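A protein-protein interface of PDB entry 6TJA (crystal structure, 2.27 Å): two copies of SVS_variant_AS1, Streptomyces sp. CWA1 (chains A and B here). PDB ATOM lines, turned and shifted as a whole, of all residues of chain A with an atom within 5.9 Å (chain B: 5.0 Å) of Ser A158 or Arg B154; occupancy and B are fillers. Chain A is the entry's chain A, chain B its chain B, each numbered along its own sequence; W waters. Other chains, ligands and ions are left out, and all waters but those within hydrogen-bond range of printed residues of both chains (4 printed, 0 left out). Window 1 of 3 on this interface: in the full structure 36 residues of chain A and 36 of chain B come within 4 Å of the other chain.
Water W1 lies within hydrogen-bond range of the side-chain hydroxyl (OG) of Ser A158 (2.7 Å), the side-chain hydroxyl (OG) of Ser B158 (3.0 Å) and the backbone carbonyl oxygen (O) of Arg B154 (3.5 Å).
Water W3 lies within hydrogen-bond range of OG of Ser B158, OG of Ser A158 and O of Arg A154.
Water W2 lies within hydrogen-bond range of O of His A151 (2.7 Å), NH1 of Arg B154 (2.8 Å) and ND1 of His B151 (3.3 Å).
Water W4 lies within hydrogen-bond range of O of His B151 (2.8 Å), NE of Arg A154 (3.0 Å) and ND1 of His A151 (3.1 Å).
The backbone carbonyl oxygen (O) of Ala A161 lies within hydrogen-bond range of the side-chain amide nitrogen (ND2) of Asn B104, at 2.9 Å.
Of the printed residues of chain B, Arg A154 touches Arg B154, Ala B155 and Ser B158.
Trp A156 touches none of the printed residues of chain B.
Of chain B, only Arg B154 and Ser B158 come within 4 Å of Ser A158.
Gly A159 touches none of the printed residues of chain B.
Of the printed residues of chain B, Trp A162 touches Asn B104.
Of chain A, only Arg A154, Ala A155, Ser A158 and Leu A184 come within 4 Å of Arg B154.
The nearest residue of chain B that does not touch Ser A158 is Asn B104 (4.9 Å).
Printed residues of chain B that touch a printed residue of chain A: Asn B104, His B151, Arg B154, Ala B155 and Ser B158.
Printed residues of chain A that touch a printed residue of chain B: His A151, Arg A154, Ala A155, Ser A158, Ala A161, Trp A162 and Leu A184.
Hydrophobic or aromatic side chains of chain A that line the printed part of chain B: His A151, Ala A155, Ala A161, Trp A162 and Leu A184.
Along chain A the printed residues that touch a printed residue of chain B span positions 151 to 184.
Among the printed residues, no Asp or Glu carboxylate lies within 4 Å of a Lys or Arg side-chain nitrogen of the other chain.
O of Arg A154 sits at hydrogen-bond distance from OG of Ser A158 (3.1 Å).
The side-chain amide oxygen of Gln B111 is in hydrogen-bond range of the backbone NH of Arg B154, at 3.2 Å.
NH2 of Arg B154 is in salt-bridge range of OE1 of Glu B115 (2.9 Å).
O of Arg B154 is in hydrogen-bond range of OG of Ser B158 (3.2 Å).
His B151 touches its own counterpart, His A151.
Arg A154 touches Ala B155, and with the chains exchanged Ala A155 touches Arg B154.
Arg A154 touches Ser B158, and with the chains exchanged Ser A158 touches Arg B154.
Ser B158 touches its own counterpart, Ser A158.
Of the 10 pairs that touch across the chains among the printed residues, 7 have their exchanged pair printed and touching as well.
Among the printed residues, pairs that only touch across the chains: His A151 with His B151, Arg A154 with Arg B154, Arg A154 with Ala B155, Arg A154 with Ser B158, Ala A155 with Arg B154, Ser A158 with Arg B154, Ser A158 with Ser B158, Trp A162 with Asn B104 and Leu A184 with Arg B154.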
ATOM      1  N   HIS A 151      18.451  25.464   7.034  1.00  0.00           N
ATOM      2  CA  HIS A 151      17.749  25.296   8.334  1.00  0.00           C
ATOM      3  C   HIS A 151      18.075  23.913   8.924  1.00  0.00           C
ATOM      4  O   HIS A 151      18.184  23.795  10.147  1.00  0.00           O
ATOM      5  CB  HIS A 151      16.242  25.520   8.141  1.00  0.00           C
ATOM      6  CG  HIS A 151      15.851  26.941   7.980  1.00  0.00           C
ATOM      7  ND1 HIS A 151      16.434  27.953   8.730  1.00  0.00           N
ATOM      8  CD2 HIS A 151      14.918  27.532   7.214  1.00  0.00           C
ATOM      9  CE1 HIS A 151      15.897  29.111   8.377  1.00  0.00           C
ATOM     10  NE2 HIS A 151      14.956  28.878   7.464  1.00  0.00           N
ATOM     11  N   HIS A 153      20.822  22.323   8.439  1.00  0.00           N
ATOM     12  CA  HIS A 153      22.192  22.531   8.802  1.00  0.00           C
ATOM     13  C   HIS A 153      22.364  23.168  10.175  1.00  0.00           C
ATOM     14  O   HIS A 153      23.152  22.729  10.938  1.00  0.00           O
ATOM     15  CB  HIS A 153      22.858  23.363   7.734  1.00  0.00           C
ATOM     16  CG  HIS A 153      24.343  23.378   7.785  1.00  0.00           C
ATOM     17  ND1 HIS A 153      25.049  24.279   8.537  1.00  0.00           N
ATOM     18  CD2 HIS A 153      25.259  22.667   7.101  1.00  0.00           C
ATOM     19  CE1 HIS A 153      26.333  24.106   8.332  1.00  0.00           C
ATOM     20  NE2 HIS A 153      26.486  23.138   7.463  1.00  0.00           N
ATOM     21  N   ARG A 154      21.605  24.204  10.464  1.00  0.00           N
ATOM     22  CA  ARG A 154      21.676  24.811  11.754  1.00  0.00           C
ATOM     23  C   ARG A 154      21.145  23.837  12.788  1.00  0.00           C
ATOM     24  O   ARG A 154      21.640  23.796  13.849  1.00  0.00           O
ATOM     25  CB  ARG A 154      20.937  26.147  11.858  1.00  0.00           C
ATOM     26  CG  ARG A 154      21.078  26.740  13.251  1.00  0.00           C
ATOM     27  CD  ARG A 154      20.813  28.209  13.460  1.00  0.00           C
ATOM     28  NE  ARG A 154      19.981  28.704  12.435  1.00  0.00           N
ATOM     29  CZ  ARG A 154      20.258  29.659  11.588  1.00  0.00           C
ATOM     30  NH1 ARG A 154      21.326  30.378  11.651  1.00  0.00           N
ATOM     31  NH2 ARG A 154      19.364  29.921  10.709  1.00  0.00           N
ATOM     32  N   ALA A 155      20.155  23.046  12.431  1.00  0.00           N
ATOM     33  CA  ALA A 155      19.564  22.068  13.373  1.00  0.00           C
ATOM     34  C   ALA A 155      20.648  21.061  13.793  1.00  0.00           C
ATOM     35  O   ALA A 155      20.784  20.835  15.005  1.00  0.00           O
ATOM     36  CB  ALA A 155      18.346  21.419  12.771  1.00  0.00           C
ATOM     37  N   TRP A 156      21.452  20.571  12.830  1.00  0.00           N
ATOM     38  CA  TRP A 156      22.557  19.616  13.089  1.00  0.00           C
ATOM     39  C   TRP A 156      23.624  20.262  13.987  1.00  0.00           C
ATOM     40  O   TRP A 156      24.061  19.611  14.984  1.00  0.00           O
ATOM     41  CB  TRP A 156      23.131  19.088  11.772  1.00  0.00           C
ATOM     42  CG  TRP A 156      24.551  18.637  11.885  1.00  0.00           C
ATOM     43  CD1 TRP A 156      25.020  17.584  12.607  1.00  0.00           C
ATOM     44  CD2 TRP A 156      25.697  19.231  11.248  1.00  0.00           C
ATOM     45  NE1 TRP A 156      26.374  17.505  12.501  1.00  0.00           N
ATOM     46  CE2 TRP A 156      26.819  18.491  11.660  1.00  0.00           C
ATOM     47  CE3 TRP A 156      25.883  20.323  10.401  1.00  0.00           C
ATOM     48  CZ2 TRP A 156      28.106  18.795  11.231  1.00  0.00           C
ATOM     49  CZ3 TRP A 156      27.155  20.632   9.993  1.00  0.00           C
ATOM     50  CH2 TRP A 156      28.249  19.893  10.429  1.00  0.00           C
ATOM     51  N   LEU A 157      24.035  21.497  13.690  1.00  0.00           N
ATOM     52  CA  LEU A 157      25.022  22.220  14.521  1.00  0.00           C
ATOM     53  C   LEU A 157      24.508  22.378  15.961  1.00  0.00           C
ATOM     54  O   LEU A 157      25.332  22.155  16.834  1.00  0.00           O
ATOM     55  CB  LEU A 157      25.390  23.559  13.895  1.00  0.00           C
ATOM     56  CG  LEU A 157      26.187  23.474  12.590  1.00  0.00           C
ATOM     57  CD1 LEU A 157      26.321  24.852  11.961  1.00  0.00           C
ATOM     58  CD2 LEU A 157      27.550  22.856  12.822  1.00  0.00           C
ATOM     59  N   SER A 158      23.233  22.716  16.196  1.00  0.00           N
ATOM     60  CA  SER A 158      22.610  22.802  17.553  1.00  0.00           C
ATOM     61  C   SER A 158      22.679  21.463  18.292  1.00  0.00           C
ATOM     62  O   SER A 158      22.760  21.465  19.515  1.00  0.00           O
ATOM     63  CB  SER A 158      21.185  23.253  17.499  1.00  0.00           C
ATOM     64  OG  SER A 158      21.133  24.513  16.865  1.00  0.00           O
ATOM     65  N   GLY A 159      22.533  20.356  17.584  1.00  0.00           N
ATOM     66  CA  GLY A 159      22.670  19.027  18.201  1.00  0.00           C
ATOM     67  C   GLY A 159      24.094  18.814  18.664  1.00  0.00           C
ATOM     68  O   GLY A 159      24.274  18.309  19.782  1.00  0.00           O
ATOM     69  N   VAL A 160      25.069  19.148  17.809  1.00  0.00           N
ATOM     70  CA  VAL A 160      26.522  18.987  18.097  1.00  0.00           C
ATOM     71  C   VAL A 160      26.869  19.866  19.309  1.00  0.00           C
ATOM     72  O   VAL A 160      27.565  19.376  20.188  1.00  0.00           O
ATOM     73  CB  VAL A 160      27.418  19.307  16.888  1.00  0.00           C
ATOM     74  CG1 VAL A 160      28.873  19.249  17.279  1.00  0.00           C
ATOM     75  CG2 VAL A 160      27.170  18.359  15.710  1.00  0.00           C
ATOM     76  N   ALA A 161      26.390  21.100  19.343  1.00  0.00           N
ATOM     77  CA  ALA A 161      26.626  22.062  20.439  1.00  0.00           C
ATOM     78  C   ALA A 161      26.116  21.469  21.752  1.00  0.00           C
ATOM     79  O   ALA A 161      26.850  21.540  22.729  1.00  0.00           O
ATOM     80  CB  ALA A 161      25.956  23.395  20.132  1.00  0.00           C
ATOM     81  N   TRP A 162      24.915  20.889  21.749  1.00  0.00           N
ATOM     82  CA  TRP A 162      24.310  20.141  22.888  1.00  0.00           C
ATOM     83  C   TRP A 162      25.228  18.984  23.299  1.00  0.00           C
ATOM     84  O   TRP A 162      25.584  18.868  24.492  1.00  0.00           O
ATOM     85  CB  TRP A 162      22.939  19.635  22.451  1.00  0.00           C
ATOM     86  CG  TRP A 162      22.051  19.017  23.488  1.00  0.00           C
ATOM     87  CD1 TRP A 162      22.341  18.615  24.758  1.00  0.00           C
ATOM     88  CD2 TRP A 162      20.674  18.670  23.262  1.00  0.00           C
ATOM     89  NE1 TRP A 162      21.225  18.100  25.360  1.00  0.00           N
ATOM     90  CE2 TRP A 162      20.185  18.131  24.468  1.00  0.00           C
ATOM     91  CE3 TRP A 162      19.802  18.837  22.179  1.00  0.00           C
ATOM     92  CZ2 TRP A 162      18.862  17.717  24.600  1.00  0.00           C
ATOM     93  CZ3 TRP A 162      18.496  18.426  22.312  1.00  0.00           C
ATOM     94  CH2 TRP A 162      18.031  17.888  23.515  1.00  0.00           C
ATOM     95  N   GLN A 163      25.598  18.151  22.335  1.00  0.00           N
ATOM     96  CA  GLN A 163      26.494  16.999  22.579  1.00  0.00           C
ATOM     97  C   GLN A 163      27.798  17.452  23.257  1.00  0.00           C
ATOM     98  O   GLN A 163      28.130  16.888  24.313  1.00  0.00           O
ATOM     99  CB  GLN A 163      26.764  16.263  21.277  1.00  0.00           C
ATOM    100  CG  GLN A 163      27.087  14.803  21.509  1.00  0.00           C
ATOM    101  CD  GLN A 163      27.985  14.276  20.421  1.00  0.00           C
ATOM    102  OE1 GLN A 163      27.548  14.035  19.287  1.00  0.00           O
ATOM    103  NE2 GLN A 163      29.252  14.116  20.780  1.00  0.00           N
ATOM    104  N   LEU A 184      19.527  15.342  15.953  1.00  0.00           N
ATOM    105  CA  LEU A 184      20.214  16.507  15.358  1.00  0.00           C
ATOM    106  C   LEU A 184      21.699  16.213  15.092  1.00  0.00           C
ATOM    107  O   LEU A 184      22.172  16.555  13.994  1.00  0.00           O
ATOM    108  CB  LEU A 184      20.008  17.668  16.331  1.00  0.00           C
ATOM    109  CG  LEU A 184      18.563  18.125  16.532  1.00  0.00           C
ATOM    110  CD1 LEU A 184      18.533  19.402  17.360  1.00  0.00           C
ATOM    111  CD2 LEU A 184      17.868  18.356  15.177  1.00  0.00           C
ATOM    112  N   ASN B 104      23.579  25.068  26.094  1.00  0.00           N
ATOM    113  CA  ASN B 104      23.500  24.320  24.804  1.00  0.00           C
ATOM    114  C   ASN B 104      22.469  23.201  24.962  1.00  0.00           C
ATOM    115  O   ASN B 104      21.717  22.975  24.052  1.00  0.00           O
ATOM    116  CB  ASN B 104      24.851  23.759  24.380  1.00  0.00           C
ATOM    117  CG  ASN B 104      25.803  24.799  23.830  1.00  0.00           C
ATOM    118  OD1 ASN B 104      25.511  25.995  23.856  1.00  0.00           O
ATOM    119  ND2 ASN B 104      26.965  24.337  23.376  1.00  0.00           N
ATOM    120  N   GLN B 111      13.895  24.079  22.271  1.00  0.00           N
ATOM    121  CA  GLN B 111      13.630  23.960  20.853  1.00  0.00           C
ATOM    122  C   GLN B 111      12.852  22.681  20.548  1.00  0.00           C
ATOM    123  O   GLN B 111      11.972  22.686  19.752  1.00  0.00           O
ATOM    124  CB  GLN B 111      14.914  24.053  20.037  1.00  0.00           C
ATOM    125  CG  GLN B 111      14.755  24.076  18.548  1.00  0.00           C
ATOM    126  CD  GLN B 111      14.012  25.265  17.997  1.00  0.00           C
ATOM    127  OE1 GLN B 111      14.101  26.358  18.483  1.00  0.00           O
ATOM    128  NE2 GLN B 111      13.301  25.038  16.959  1.00  0.00           N
ATOM    129  N   GLU B 115       8.856  22.044  18.897  1.00  0.00           N
ATOM    130  CA  GLU B 115       8.674  21.234  17.661  1.00  0.00           C
ATOM    131  C   GLU B 115       7.884  19.947  17.960  1.00  0.00           C
ATOM    132  O   GLU B 115       7.387  19.318  16.995  1.00  0.00           O
ATOM    133  CB  GLU B 115      10.033  20.869  17.057  1.00  0.00           C
ATOM    134  CG  GLU B 115      10.827  22.065  16.555  1.00  0.00           C
ATOM    135  CD  GLU B 115      11.987  21.762  15.621  1.00  0.00           C
ATOM    136  OE1 GLU B 115      13.042  22.373  15.805  1.00  0.00           O
ATOM    137  OE2 GLU B 115      11.838  20.927  14.705  1.00  0.00           O
ATOM    138  N   VAL B 150       9.603  28.094  13.813  1.00  0.00           N
ATOM    139  CA  VAL B 150      10.457  27.072  14.492  1.00  0.00           C
ATOM    140  C   VAL B 150      11.907  27.349  14.107  1.00  0.00           C
ATOM    141  O   VAL B 150      12.753  27.388  14.996  1.00  0.00           O
ATOM    142  CB  VAL B 150      10.033  25.634  14.110  1.00  0.00           C
ATOM    143  CG1 VAL B 150      11.139  24.621  14.336  1.00  0.00           C
ATOM    144  CG2 VAL B 150       8.782  25.196  14.841  1.00  0.00           C
ATOM    145  N   HIS B 151      12.175  27.537  12.815  1.00  0.00           N
ATOM    146  CA  HIS B 151      13.544  27.736  12.268  1.00  0.00           C
ATOM    147  C   HIS B 151      14.092  29.088  12.738  1.00  0.00           C
ATOM    148  O   HIS B 151      15.253  29.150  13.116  1.00  0.00           O
ATOM    149  CB  HIS B 151      13.557  27.639  10.732  1.00  0.00           C
ATOM    150  CG  HIS B 151      13.295  26.270  10.216  1.00  0.00           C
ATOM    151  ND1 HIS B 151      13.778  25.135  10.869  1.00  0.00           N
ATOM    152  CD2 HIS B 151      12.616  25.829   9.124  1.00  0.00           C
ATOM    153  CE1 HIS B 151      13.384  24.055  10.213  1.00  0.00           C
ATOM    154  NE2 HIS B 151      12.677  24.450   9.139  1.00  0.00           N
ATOM    155  N   ALA B 152      13.282  30.137  12.684  1.00  0.00           N
ATOM    156  CA  ALA B 152      13.654  31.460  13.216  1.00  0.00           C
ATOM    157  C   ALA B 152      14.009  31.347  14.704  1.00  0.00           C
ATOM    158  O   ALA B 152      14.930  32.054  15.126  1.00  0.00           O
ATOM    159  CB  ALA B 152      12.531  32.458  13.009  1.00  0.00           C
ATOM    160  N   HIS B 153      13.256  30.552  15.458  1.00  0.00           N
ATOM    161  CA  HIS B 153      13.433  30.349  16.922  1.00  0.00           C
ATOM    162  C   HIS B 153      14.800  29.698  17.191  1.00  0.00           C
ATOM    163  O   HIS B 153      15.558  30.209  18.033  1.00  0.00           O
ATOM    164  CB  HIS B 153      12.258  29.539  17.459  1.00  0.00           C
ATOM    165  CG  HIS B 153      12.211  29.445  18.952  1.00  0.00           C
ATOM    166  ND1 HIS B 153      12.983  28.532  19.655  1.00  0.00           N
ATOM    167  CD2 HIS B 153      11.439  30.097  19.863  1.00  0.00           C
ATOM    168  CE1 HIS B 153      12.695  28.637  20.940  1.00  0.00           C
ATOM    169  NE2 HIS B 153      11.763  29.600  21.097  1.00  0.00           N
ATOM    170  N   ARG B 154      15.142  28.640  16.452  1.00  0.00           N
ATOM    171  CA  ARG B 154      16.461  27.963  16.570  1.00  0.00           C
ATOM    172  C   ARG B 154      17.571  28.964  16.232  1.00  0.00           C
ATOM    173  O   ARG B 154      18.610  28.948  16.920  1.00  0.00           O
ATOM    174  CB  ARG B 154      16.595  26.734  15.668  1.00  0.00           C
ATOM    175  CG  ARG B 154      17.891  25.977  15.914  1.00  0.00           C
ATOM    176  CD  ARG B 154      18.081  24.742  15.069  1.00  0.00           C
ATOM    177  NE  ARG B 154      17.457  23.603  15.723  1.00  0.00           N
ATOM    178  CZ  ARG B 154      16.427  22.933  15.245  1.00  0.00           C
ATOM    179  NH1 ARG B 154      15.874  23.222  14.068  1.00  0.00           N
ATOM    180  NH2 ARG B 154      15.938  21.970  15.977  1.00  0.00           N
ATOM    181  N   ALA B 155      17.403  29.790  15.193  1.00  0.00           N
ATOM    182  CA  ALA B 155      18.452  30.748  14.761  1.00  0.00           C
ATOM    183  C   ALA B 155      18.721  31.732  15.912  1.00  0.00           C
ATOM    184  O   ALA B 155      19.867  32.031  16.193  1.00  0.00           O
ATOM    185  CB  ALA B 155      18.006  31.444  13.512  1.00  0.00           C
ATOM    186  N   TRP B 156      17.685  32.202  16.597  1.00  0.00           N
ATOM    187  CA  TRP B 156      17.844  33.105  17.757  1.00  0.00           C
ATOM    188  C   TRP B 156      18.601  32.335  18.854  1.00  0.00           C
ATOM    189  O   TRP B 156      19.611  32.845  19.374  1.00  0.00           O
ATOM    190  CB  TRP B 156      16.482  33.645  18.201  1.00  0.00           C
ATOM    191  CG  TRP B 156      16.433  34.054  19.636  1.00  0.00           C
ATOM    192  CD1 TRP B 156      17.058  35.129  20.197  1.00  0.00           C
ATOM    193  CD2 TRP B 156      15.721  33.392  20.705  1.00  0.00           C
ATOM    194  NE1 TRP B 156      16.829  35.151  21.549  1.00  0.00           N
ATOM    195  CE2 TRP B 156      15.994  34.118  21.892  1.00  0.00           C
ATOM    196  CE3 TRP B 156      14.872  32.290  20.785  1.00  0.00           C
ATOM    197  CZ2 TRP B 156      15.483  33.743  23.133  1.00  0.00           C
ATOM    198  CZ3 TRP B 156      14.342  31.933  22.011  1.00  0.00           C
ATOM    199  CH2 TRP B 156      14.650  32.646  23.172  1.00  0.00           C
ATOM    200  N   LEU B 157      18.212  31.103  19.136  1.00  0.00           N
ATOM    201  CA  LEU B 157      18.856  30.302  20.203  1.00  0.00           C
ATOM    202  C   LEU B 157      20.331  30.134  19.865  1.00  0.00           C
ATOM    203  O   LEU B 157      21.127  30.337  20.776  1.00  0.00           O
ATOM    204  CB  LEU B 157      18.145  28.967  20.358  1.00  0.00           C
ATOM    205  CG  LEU B 157      16.850  28.966  21.161  1.00  0.00           C
ATOM    206  CD1 LEU B 157      16.373  27.534  21.346  1.00  0.00           C
ATOM    207  CD2 LEU B 157      17.006  29.621  22.527  1.00  0.00           C
ATOM    208  N   SER B 158      20.703  29.886  18.598  1.00  0.00           N
ATOM    209  CA  SER B 158      22.119  29.800  18.130  1.00  0.00           C
ATOM    210  C   SER B 158      22.882  31.100  18.461  1.00  0.00           C
ATOM    211  O   SER B 158      24.128  31.066  18.758  1.00  0.00           O
ATOM    212  CB  SER B 158      22.186  29.499  16.643  1.00  0.00           C
ATOM    213  OG  SER B 158      21.718  28.164  16.387  1.00  0.00           O
HETATM  214  O   HOH W   1      20.396  26.460  18.543  1.00  0.00           O
HETATM  215  O   HOH W   2      16.793  25.075  12.130  1.00  0.00           O
HETATM  216  O   HOH W   3      23.269  26.124  15.596  1.00  0.00           O
HETATM  217  O   HOH W   4      17.261  27.785  11.747  1.00  0.00           O
